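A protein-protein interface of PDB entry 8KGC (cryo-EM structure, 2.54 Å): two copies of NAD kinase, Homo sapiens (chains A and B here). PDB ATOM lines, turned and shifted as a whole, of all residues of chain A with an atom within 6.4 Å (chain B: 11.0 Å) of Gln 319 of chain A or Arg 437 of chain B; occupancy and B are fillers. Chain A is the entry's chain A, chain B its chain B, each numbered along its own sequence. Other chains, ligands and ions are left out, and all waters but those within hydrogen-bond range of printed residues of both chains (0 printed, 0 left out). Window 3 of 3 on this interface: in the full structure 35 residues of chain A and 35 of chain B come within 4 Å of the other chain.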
ATOM      1  N   LEU A 303     -12.996  14.684  29.572  1.00  0.00           N
ATOM      2  CA  LEU A 303     -14.064  14.649  28.576  1.00  0.00           C
ATOM      3  C   LEU A 303     -14.509  13.229  28.253  1.00  0.00           C
ATOM      4  O   LEU A 303     -13.687  12.344  28.004  1.00  0.00           O
ATOM      5  CB  LEU A 303     -13.590  15.354  27.302  1.00  0.00           C
ATOM      6  CG  LEU A 303     -12.205  14.977  26.767  1.00  0.00           C
ATOM      7  CD1 LEU A 303     -12.296  13.940  25.654  1.00  0.00           C
ATOM      8  CD2 LEU A 303     -11.456  16.213  26.295  1.00  0.00           C
ATOM      9  N   SER A 304     -15.823  13.017  28.277  1.00  0.00           N
ATOM     10  CA  SER A 304     -16.416  11.700  28.126  1.00  0.00           C
ATOM     11  C   SER A 304     -17.015  11.536  26.732  1.00  0.00           C
ATOM     12  O   SER A 304     -16.888  12.398  25.859  1.00  0.00           O
ATOM     13  CB  SER A 304     -17.477  11.470  29.204  1.00  0.00           C
ATOM     14  OG  SER A 304     -18.497  12.449  29.128  1.00  0.00           O
ATOM     15  N   ASN A 305     -17.677  10.401  26.526  1.00  0.00           N
ATOM     16  CA  ASN A 305     -18.319  10.068  25.262  1.00  0.00           C
ATOM     17  C   ASN A 305     -19.828  10.146  25.427  1.00  0.00           C
ATOM     18  O   ASN A 305     -20.382   9.601  26.386  1.00  0.00           O
ATOM     19  CB  ASN A 305     -17.910   8.673  24.791  1.00  0.00           C
ATOM     20  CG  ASN A 305     -16.434   8.576  24.476  1.00  0.00           C
ATOM     21  OD1 ASN A 305     -15.643   9.420  24.895  1.00  0.00           O
ATOM     22  ND2 ASN A 305     -16.055   7.545  23.732  1.00  0.00           N
ATOM     23  N   VAL A 306     -20.486  10.823  24.490  1.00  0.00           N
ATOM     24  CA  VAL A 306     -21.932  11.003  24.506  1.00  0.00           C
ATOM     25  C   VAL A 306     -22.483  10.584  23.151  1.00  0.00           C
ATOM     26  O   VAL A 306     -21.970  11.009  22.110  1.00  0.00           O
ATOM     27  CB  VAL A 306     -22.317  12.460  24.826  1.00  0.00           C
ATOM     28  CG1 VAL A 306     -23.701  12.768  24.313  1.00  0.00           C
ATOM     29  CG2 VAL A 306     -22.237  12.708  26.318  1.00  0.00           C
ATOM     30  N   ASP A 307     -23.521   9.753  23.164  1.00  0.00           N
ATOM     31  CA  ASP A 307     -24.147   9.256  21.948  1.00  0.00           C
ATOM     32  C   ASP A 307     -25.359  10.108  21.599  1.00  0.00           C
ATOM     33  O   ASP A 307     -26.169  10.441  22.470  1.00  0.00           O
ATOM     34  CB  ASP A 307     -24.569   7.796  22.107  1.00  0.00           C
ATOM     35  CG  ASP A 307     -23.396   6.875  22.368  1.00  0.00           C
ATOM     36  OD1 ASP A 307     -22.276   7.197  21.920  1.00  0.00           O
ATOM     37  OD2 ASP A 307     -23.593   5.829  23.020  1.00  0.00           O
ATOM     38  N   LEU A 314     -28.755   5.835  16.171  1.00  0.00           N
ATOM     39  CA  LEU A 314     -27.468   6.380  16.578  1.00  0.00           C
ATOM     40  C   LEU A 314     -26.743   6.957  15.372  1.00  0.00           C
ATOM     41  O   LEU A 314     -26.347   6.216  14.469  1.00  0.00           O
ATOM     42  CB  LEU A 314     -26.617   5.301  17.248  1.00  0.00           C
ATOM     43  CG  LEU A 314     -25.188   5.698  17.615  1.00  0.00           C
ATOM     44  CD1 LEU A 314     -25.197   6.857  18.591  1.00  0.00           C
ATOM     45  CD2 LEU A 314     -24.436   4.513  18.194  1.00  0.00           C
ATOM     46  N   THR A 316     -24.095   9.565  15.669  1.00  0.00           N
ATOM     47  CA  THR A 316     -22.708   9.906  15.952  1.00  0.00           C
ATOM     48  C   THR A 316     -22.456   9.782  17.447  1.00  0.00           C
ATOM     49  O   THR A 316     -23.380   9.610  18.245  1.00  0.00           O
ATOM     50  CB  THR A 316     -22.367  11.319  15.471  1.00  0.00           C
ATOM     51  OG1 THR A 316     -21.012  11.626  15.818  1.00  0.00           O
ATOM     52  CG2 THR A 316     -23.289  12.334  16.121  1.00  0.00           C
ATOM     53  N   THR A 317     -21.180   9.872  17.810  1.00  0.00           N
ATOM     54  CA  THR A 317     -20.741   9.888  19.202  1.00  0.00           C
ATOM     55  C   THR A 317     -19.763  11.041  19.359  1.00  0.00           C
ATOM     56  O   THR A 317     -18.696  11.040  18.739  1.00  0.00           O
ATOM     57  CB  THR A 317     -20.090   8.563  19.598  1.00  0.00           C
ATOM     58  OG1 THR A 317     -21.068   7.517  19.557  1.00  0.00           O
ATOM     59  CG2 THR A 317     -19.507   8.653  20.996  1.00  0.00           C
ATOM     60  N   VAL A 318     -20.119  12.019  20.182  1.00  0.00           N
ATOM     61  CA  VAL A 318     -19.298  13.215  20.332  1.00  0.00           C
ATOM     62  C   VAL A 318     -18.185  12.940  21.335  1.00  0.00           C
ATOM     63  O   VAL A 318     -18.419  12.377  22.411  1.00  0.00           O
ATOM     64  CB  VAL A 318     -20.156  14.420  20.751  1.00  0.00           C
ATOM     65  CG1 VAL A 318     -21.200  14.713  19.692  1.00  0.00           C
ATOM     66  CG2 VAL A 318     -20.831  14.175  22.083  1.00  0.00           C
ATOM     67  N   GLN A 319     -16.960  13.301  20.963  1.00  0.00           N
ATOM     68  CA  GLN A 319     -15.806  13.204  21.847  1.00  0.00           C
ATOM     69  C   GLN A 319     -15.081  14.538  21.825  1.00  0.00           C
ATOM     70  O   GLN A 319     -14.583  14.958  20.776  1.00  0.00           O
ATOM     71  CB  GLN A 319     -14.866  12.074  21.421  1.00  0.00           C
ATOM     72  CG  GLN A 319     -15.515  10.705  21.388  1.00  0.00           C
ATOM     73  CD  GLN A 319     -14.521   9.602  21.101  1.00  0.00           C
ATOM     74  OE1 GLN A 319     -13.324   9.748  21.352  1.00  0.00           O
ATOM     75  NE2 GLN A 319     -15.009   8.488  20.569  1.00  0.00           N
ATOM     76  N   GLY A 320     -15.024  15.196  22.968  1.00  0.00           N
ATOM     77  CA  GLY A 320     -14.414  16.502  23.064  1.00  0.00           C
ATOM     78  C   GLY A 320     -15.037  17.284  24.201  1.00  0.00           C
ATOM     79  O   GLY A 320     -15.579  16.709  25.138  1.00  0.00           O
ATOM     80  N   ASP A 321     -14.948  18.611  24.091  1.00  0.00           N
ATOM     81  CA  ASP A 321     -15.475  19.464  25.149  1.00  0.00           C
ATOM     82  C   ASP A 321     -16.985  19.329  25.285  1.00  0.00           C
ATOM     83  O   ASP A 321     -17.521  19.506  26.384  1.00  0.00           O
ATOM     84  CB  ASP A 321     -15.084  20.919  24.903  1.00  0.00           C
ATOM     85  CG  ASP A 321     -13.613  21.171  25.151  1.00  0.00           C
ATOM     86  OD1 ASP A 321     -12.899  20.207  25.497  1.00  0.00           O
ATOM     87  OD2 ASP A 321     -13.172  22.329  25.004  1.00  0.00           O
ATOM     88  N   GLY A 322     -17.689  19.020  24.202  1.00  0.00           N
ATOM     89  CA  GLY A 322     -19.092  18.678  24.357  1.00  0.00           C
ATOM     90  C   GLY A 322     -19.870  18.902  23.073  1.00  0.00           C
ATOM     91  O   GLY A 322     -19.309  18.908  21.983  1.00  0.00           O
ATOM     92  N   ILE A 355     -18.444  21.203  20.532  1.00  0.00           N
ATOM     93  CA  ILE A 355     -17.478  22.042  21.229  1.00  0.00           C
ATOM     94  C   ILE A 355     -16.174  21.263  21.292  1.00  0.00           C
ATOM     95  O   ILE A 355     -16.070  20.276  22.030  1.00  0.00           O
ATOM     96  CB  ILE A 355     -17.955  22.417  22.635  1.00  0.00           C
ATOM     97  CG1 ILE A 355     -19.402  22.896  22.617  1.00  0.00           C
ATOM     98  CG2 ILE A 355     -17.061  23.490  23.224  1.00  0.00           C
ATOM     99  CD1 ILE A 355     -19.926  23.216  23.994  1.00  0.00           C
ATOM    100  N   CYS A 356     -15.182  21.713  20.520  1.00  0.00           N
ATOM    101  CA  CYS A 356     -13.847  21.132  20.436  1.00  0.00           C
ATOM    102  C   CYS A 356     -13.904  19.625  20.225  1.00  0.00           C
ATOM    103  O   CYS A 356     -13.501  18.861  21.110  1.00  0.00           O
ATOM    104  CB  CYS A 356     -13.043  21.459  21.694  1.00  0.00           C
ATOM    105  SG  CYS A 356     -12.726  23.220  21.921  1.00  0.00           S
ATOM    106  N   PRO A 357     -14.392  19.157  19.078  1.00  0.00           N
ATOM    107  CA  PRO A 357     -14.447  17.713  18.842  1.00  0.00           C
ATOM    108  C   PRO A 357     -13.055  17.122  18.704  1.00  0.00           C
ATOM    109  O   PRO A 357     -12.118  17.778  18.244  1.00  0.00           O
ATOM    110  CB  PRO A 357     -15.228  17.601  17.531  1.00  0.00           C
ATOM    111  CG  PRO A 357     -14.929  18.873  16.827  1.00  0.00           C
ATOM    112  CD  PRO A 357     -14.823  19.923  17.897  1.00  0.00           C
ATOM    113  N   HIS A 358     -12.929  15.858  19.110  1.00  0.00           N
ATOM    114  CA  HIS A 358     -11.638  15.184  19.023  1.00  0.00           C
ATOM    115  C   HIS A 358     -11.216  14.984  17.574  1.00  0.00           C
ATOM    116  O   HIS A 358     -10.035  15.128  17.240  1.00  0.00           O
ATOM    117  CB  HIS A 358     -11.694  13.847  19.759  1.00  0.00           C
ATOM    118  CG  HIS A 358     -10.365  13.170  19.880  1.00  0.00           C
ATOM    119  ND1 HIS A 358      -9.320  13.706  20.599  1.00  0.00           N
ATOM    120  CD2 HIS A 358      -9.912  11.998  19.375  1.00  0.00           C
ATOM    121  CE1 HIS A 358      -8.279  12.895  20.532  1.00  0.00           C
ATOM    122  NE2 HIS A 358      -8.612  11.851  19.795  1.00  0.00           N
ATOM    123  N   SER A 359     -12.162  14.650  16.701  1.00  0.00           N
ATOM    124  CA  SER A 359     -11.853  14.433  15.298  1.00  0.00           C
ATOM    125  C   SER A 359     -11.759  15.760  14.554  1.00  0.00           C
ATOM    126  O   SER A 359     -12.303  16.783  14.977  1.00  0.00           O
ATOM    127  CB  SER A 359     -12.911  13.544  14.646  1.00  0.00           C
ATOM    128  OG  SER A 359     -14.188  14.150  14.710  1.00  0.00           O
ATOM    129  N   PHE A 362     -15.487  16.698  12.268  1.00  0.00           N
ATOM    130  CA  PHE A 362     -16.801  16.884  12.882  1.00  0.00           C
ATOM    131  C   PHE A 362     -17.275  18.297  12.560  1.00  0.00           C
ATOM    132  O   PHE A 362     -17.193  19.223  13.370  1.00  0.00           O
ATOM    133  CB  PHE A 362     -16.736  16.630  14.383  1.00  0.00           C
ATOM    134  CG  PHE A 362     -18.080  16.423  15.032  1.00  0.00           C
ATOM    135  CD1 PHE A 362     -19.255  16.750  14.374  1.00  0.00           C
ATOM    136  CD2 PHE A 362     -18.166  15.900  16.306  1.00  0.00           C
ATOM    137  CE1 PHE A 362     -20.480  16.562  14.976  1.00  0.00           C
ATOM    138  CE2 PHE A 362     -19.389  15.710  16.911  1.00  0.00           C
ATOM    139  CZ  PHE A 362     -20.547  16.040  16.245  1.00  0.00           C
ATOM    140  N   SER A 378     -22.631   7.501  26.784  1.00  0.00           N
ATOM    141  CA  SER A 378     -22.175   6.260  26.183  1.00  0.00           C
ATOM    142  C   SER A 378     -22.181   5.150  27.231  1.00  0.00           C
ATOM    143  O   SER A 378     -21.849   5.395  28.396  1.00  0.00           O
ATOM    144  CB  SER A 378     -20.772   6.429  25.601  1.00  0.00           C
ATOM    145  OG  SER A 378     -20.300   5.213  25.050  1.00  0.00           O
ATOM    146  N   LEU B 428     -22.919  10.611   4.707  1.00  0.00           N
ATOM    147  CA  LEU B 428     -21.942  11.446   5.398  1.00  0.00           C
ATOM    148  C   LEU B 428     -20.797  10.609   5.950  1.00  0.00           C
ATOM    149  O   LEU B 428     -19.629  11.008   5.870  1.00  0.00           O
ATOM    150  CB  LEU B 428     -22.617  12.225   6.526  1.00  0.00           C
ATOM    151  CG  LEU B 428     -23.303  13.537   6.153  1.00  0.00           C
ATOM    152  CD1 LEU B 428     -23.986  14.136   7.367  1.00  0.00           C
ATOM    153  CD2 LEU B 428     -22.290  14.506   5.581  1.00  0.00           C
ATOM    154  N   ALA B 429     -21.113   9.444   6.516  1.00  0.00           N
ATOM    155  CA  ALA B 429     -20.074   8.584   7.070  1.00  0.00           C
ATOM    156  C   ALA B 429     -19.195   7.978   5.984  1.00  0.00           C
ATOM    157  O   ALA B 429     -17.994   7.784   6.202  1.00  0.00           O
ATOM    158  CB  ALA B 429     -20.704   7.479   7.917  1.00  0.00           C
ATOM    159  N   LEU B 432     -18.157  11.293   2.687  1.00  0.00           N
ATOM    160  CA  LEU B 432     -17.191  12.018   3.495  1.00  0.00           C
ATOM    161  C   LEU B 432     -16.701  11.091   4.604  1.00  0.00           C
ATOM    162  O   LEU B 432     -16.968   9.887   4.598  1.00  0.00           O
ATOM    163  CB  LEU B 432     -17.803  13.301   4.053  1.00  0.00           C
ATOM    164  CG  LEU B 432     -17.966  14.502   3.118  1.00  0.00           C
ATOM    165  CD1 LEU B 432     -16.723  14.691   2.263  1.00  0.00           C
ATOM    166  CD2 LEU B 432     -19.208  14.373   2.253  1.00  0.00           C
ATOM    167  N   HIS B 433     -15.976  11.639   5.570  1.00  0.00           N
ATOM    168  CA  HIS B 433     -15.584  10.908   6.769  1.00  0.00           C
ATOM    169  C   HIS B 433     -16.004  11.688   8.001  1.00  0.00           C
ATOM    170  O   HIS B 433     -15.242  11.885   8.948  1.00  0.00           O
ATOM    171  CB  HIS B 433     -14.089  10.615   6.766  1.00  0.00           C
ATOM    172  CG  HIS B 433     -13.685   9.580   5.762  1.00  0.00           C
ATOM    173  ND1 HIS B 433     -13.747   9.797   4.403  1.00  0.00           N
ATOM    174  CD2 HIS B 433     -13.230   8.315   5.920  1.00  0.00           C
ATOM    175  CE1 HIS B 433     -13.339   8.715   3.767  1.00  0.00           C
ATOM    176  NE2 HIS B 433     -13.020   7.800   4.664  1.00  0.00           N
ATOM    177  N   TRP B 434     -17.252  12.153   7.983  1.00  0.00           N
ATOM    178  CA  TRP B 434     -17.797  12.988   9.042  1.00  0.00           C
ATOM    179  C   TRP B 434     -17.820  12.257  10.377  1.00  0.00           C
ATOM    180  O   TRP B 434     -18.541  11.266  10.538  1.00  0.00           O
ATOM    181  CB  TRP B 434     -19.203  13.453   8.662  1.00  0.00           C
ATOM    182  CG  TRP B 434     -19.890  14.241   9.721  1.00  0.00           C
ATOM    183  CD1 TRP B 434     -19.722  15.564   9.995  1.00  0.00           C
ATOM    184  CD2 TRP B 434     -20.869  13.760  10.643  1.00  0.00           C
ATOM    185  NE1 TRP B 434     -20.533  15.936  11.038  1.00  0.00           N
ATOM    186  CE2 TRP B 434     -21.248  14.845  11.453  1.00  0.00           C
ATOM    187  CE3 TRP B 434     -21.461  12.514  10.865  1.00  0.00           C
ATOM    188  CZ2 TRP B 434     -22.190  14.724  12.467  1.00  0.00           C
ATOM    189  CZ3 TRP B 434     -22.395  12.397  11.872  1.00  0.00           C
ATOM    190  CH2 TRP B 434     -22.752  13.495  12.660  1.00  0.00           C
ATOM    191  N   ASN B 435     -17.029  12.744  11.334  1.00  0.00           N
ATOM    192  CA  ASN B 435     -16.988  12.214  12.697  1.00  0.00           C
ATOM    193  C   ASN B 435     -16.610  10.732  12.704  1.00  0.00           C
ATOM    194  O   ASN B 435     -17.379   9.864  13.120  1.00  0.00           O
ATOM    195  CB  ASN B 435     -18.325  12.446  13.410  1.00  0.00           C
ATOM    196  CG  ASN B 435     -18.187  12.462  14.919  1.00  0.00           C
ATOM    197  OD1 ASN B 435     -19.093  12.893  15.627  1.00  0.00           O
ATOM    198  ND2 ASN B 435     -17.046  12.004  15.418  1.00  0.00           N
ATOM    199  N   VAL B 436     -15.397  10.453  12.234  1.00  0.00           N
ATOM    200  CA  VAL B 436     -14.829   9.112  12.272  1.00  0.00           C
ATOM    201  C   VAL B 436     -13.787   9.060  13.381  1.00  0.00           C
ATOM    202  O   VAL B 436     -12.927   9.946  13.481  1.00  0.00           O
ATOM    203  CB  VAL B 436     -14.223   8.716  10.914  1.00  0.00           C
ATOM    204  CG1 VAL B 436     -15.328   8.456   9.904  1.00  0.00           C
ATOM    205  CG2 VAL B 436     -13.282   9.795  10.408  1.00  0.00           C
ATOM    206  N   ARG B 437     -13.873   8.038  14.223  1.00  0.00           N
ATOM    207  CA  ARG B 437     -12.971   7.899  15.359  1.00  0.00           C
ATOM    208  C   ARG B 437     -11.551   7.587  14.904  1.00  0.00           C
ATOM    209  O   ARG B 437     -10.698   8.473  14.847  1.00  0.00           O
ATOM    210  CB  ARG B 437     -13.473   6.810  16.307  1.00  0.00           C
ATOM    211  CG  ARG B 437     -14.921   6.984  16.735  1.00  0.00           C
ATOM    212  CD  ARG B 437     -15.359   5.869  17.667  1.00  0.00           C
ATOM    213  NE  ARG B 437     -16.784   5.938  17.968  1.00  0.00           N
ATOM    214  CZ  ARG B 437     -17.424   5.092  18.763  1.00  0.00           C
ATOM    215  NH1 ARG B 437     -16.793   4.098  19.366  1.00  0.00           N
ATOM    216  NH2 ARG B 437     -18.731   5.246  18.958  1.00  0.00           N
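ND2 of Asn 305 of chain A lies close to NE2 of Gln 319 of chain A (3.5 Å).
OD1 of Asp 307 of chain A is in hydrogen-bond range of OG1 of Thr 317 of chain A (2.7 Å).
The backbone carbonyl oxygen of Gln 319 of chain A sits at hydrogen-bond distance from the backbone NH of His 358 of chain A (2.5 Å).
O of Leu 428 of chain B is in hydrogen-bond range of N of Trp 434 of chain B, at 3.4 Å.
OG1 of Thr 317 of chain A sits at hydrogen-bond distance from NH2 of Arg 437 of chain B.
The side-chain hydroxyl of Thr 316 of chain A lies close to the side-chain amide oxygen of Asn 435 of chain B (2.3 Å).
No position is printed for both chains.
CB of Thr 316 of chain A touches CH2 of Trp 434 of chain B (3.6 Å).
OD1 of Asn 435 of chain B touches O of Thr 317 of chain A (3.6 Å).
Gln 319 of chain A touches Arg 437 of chain B (NE2 to CD, 3.9 Å).
Asn 435 of chain B touches Ser 359 of chain A.
Val 436 of chain B touches Ser 359 of chain A.
Trp 434 of chain B touches Phe 362 of chain A.
Asn 435 of chain B touches Phe 362 of chain A (OD1 to CE2, 3.1 Å).
Hydrophobic or aromatic side chains of chain B that line the printed part of chain A: Trp 434.
Along chain B the printed residues that touch a printed residue of chain A span positions 434 to 437.
Of the 20 printed residues of chain A, 5 touch a printed residue of chain B.
Printed residues of chain A that touch a printed residue of chain B: Thr 316, Thr 317, Gln 319, Ser 359 and Phe 362.
Hydrophobic or aromatic side chains of chain A within 4 Å of the printed part of chain B: Phe 362.
Among the printed residues, no Asp or Glu carboxylate lies within 4 Å of a Lys or Arg side-chain nitrogen of the other chain.
Of chain B, only Arg 437 comes within 4 Å of Gln 319 of chain A.
Thr 317 of chain A touches just these residues of chain B: Asn 435 (3.6 Å) and Arg 437 (3.3 Å).
No residue of chain B comes within 4 Å of Val 318 of chain A.
No residue of chain B comes within 4 Å of Gly 320 of chain A.
No residue of chain B comes within 4 Å of Gly 322 of chain A.
No residue of chain B comes within 4 Å of Pro 357 of chain A.
Of the printed residues of chain B, Ser 359 of chain A touches Asn 435 and Val 436.
Of the printed residues of chain A, Trp 434 of chain B touches Thr 316 (3.6 Å) and Phe 362 (3.5 Å).
Of the printed residues of chain A, Val 436 of chain B touches Ser 359 (3.8 Å).
Of the printed residues of chain B, Thr 316 of chain A touches Trp 434 (3.6 Å) and Asn 435 (2.3 Å).
Of the printed residues of chain A, Asn 435 of chain B touches Thr 316, Thr 317, Ser 359 and Phe 362.
The nearest residue of chain A that does not touch Arg 437 of chain B is Asp 307 of chain A (5.0 Å).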
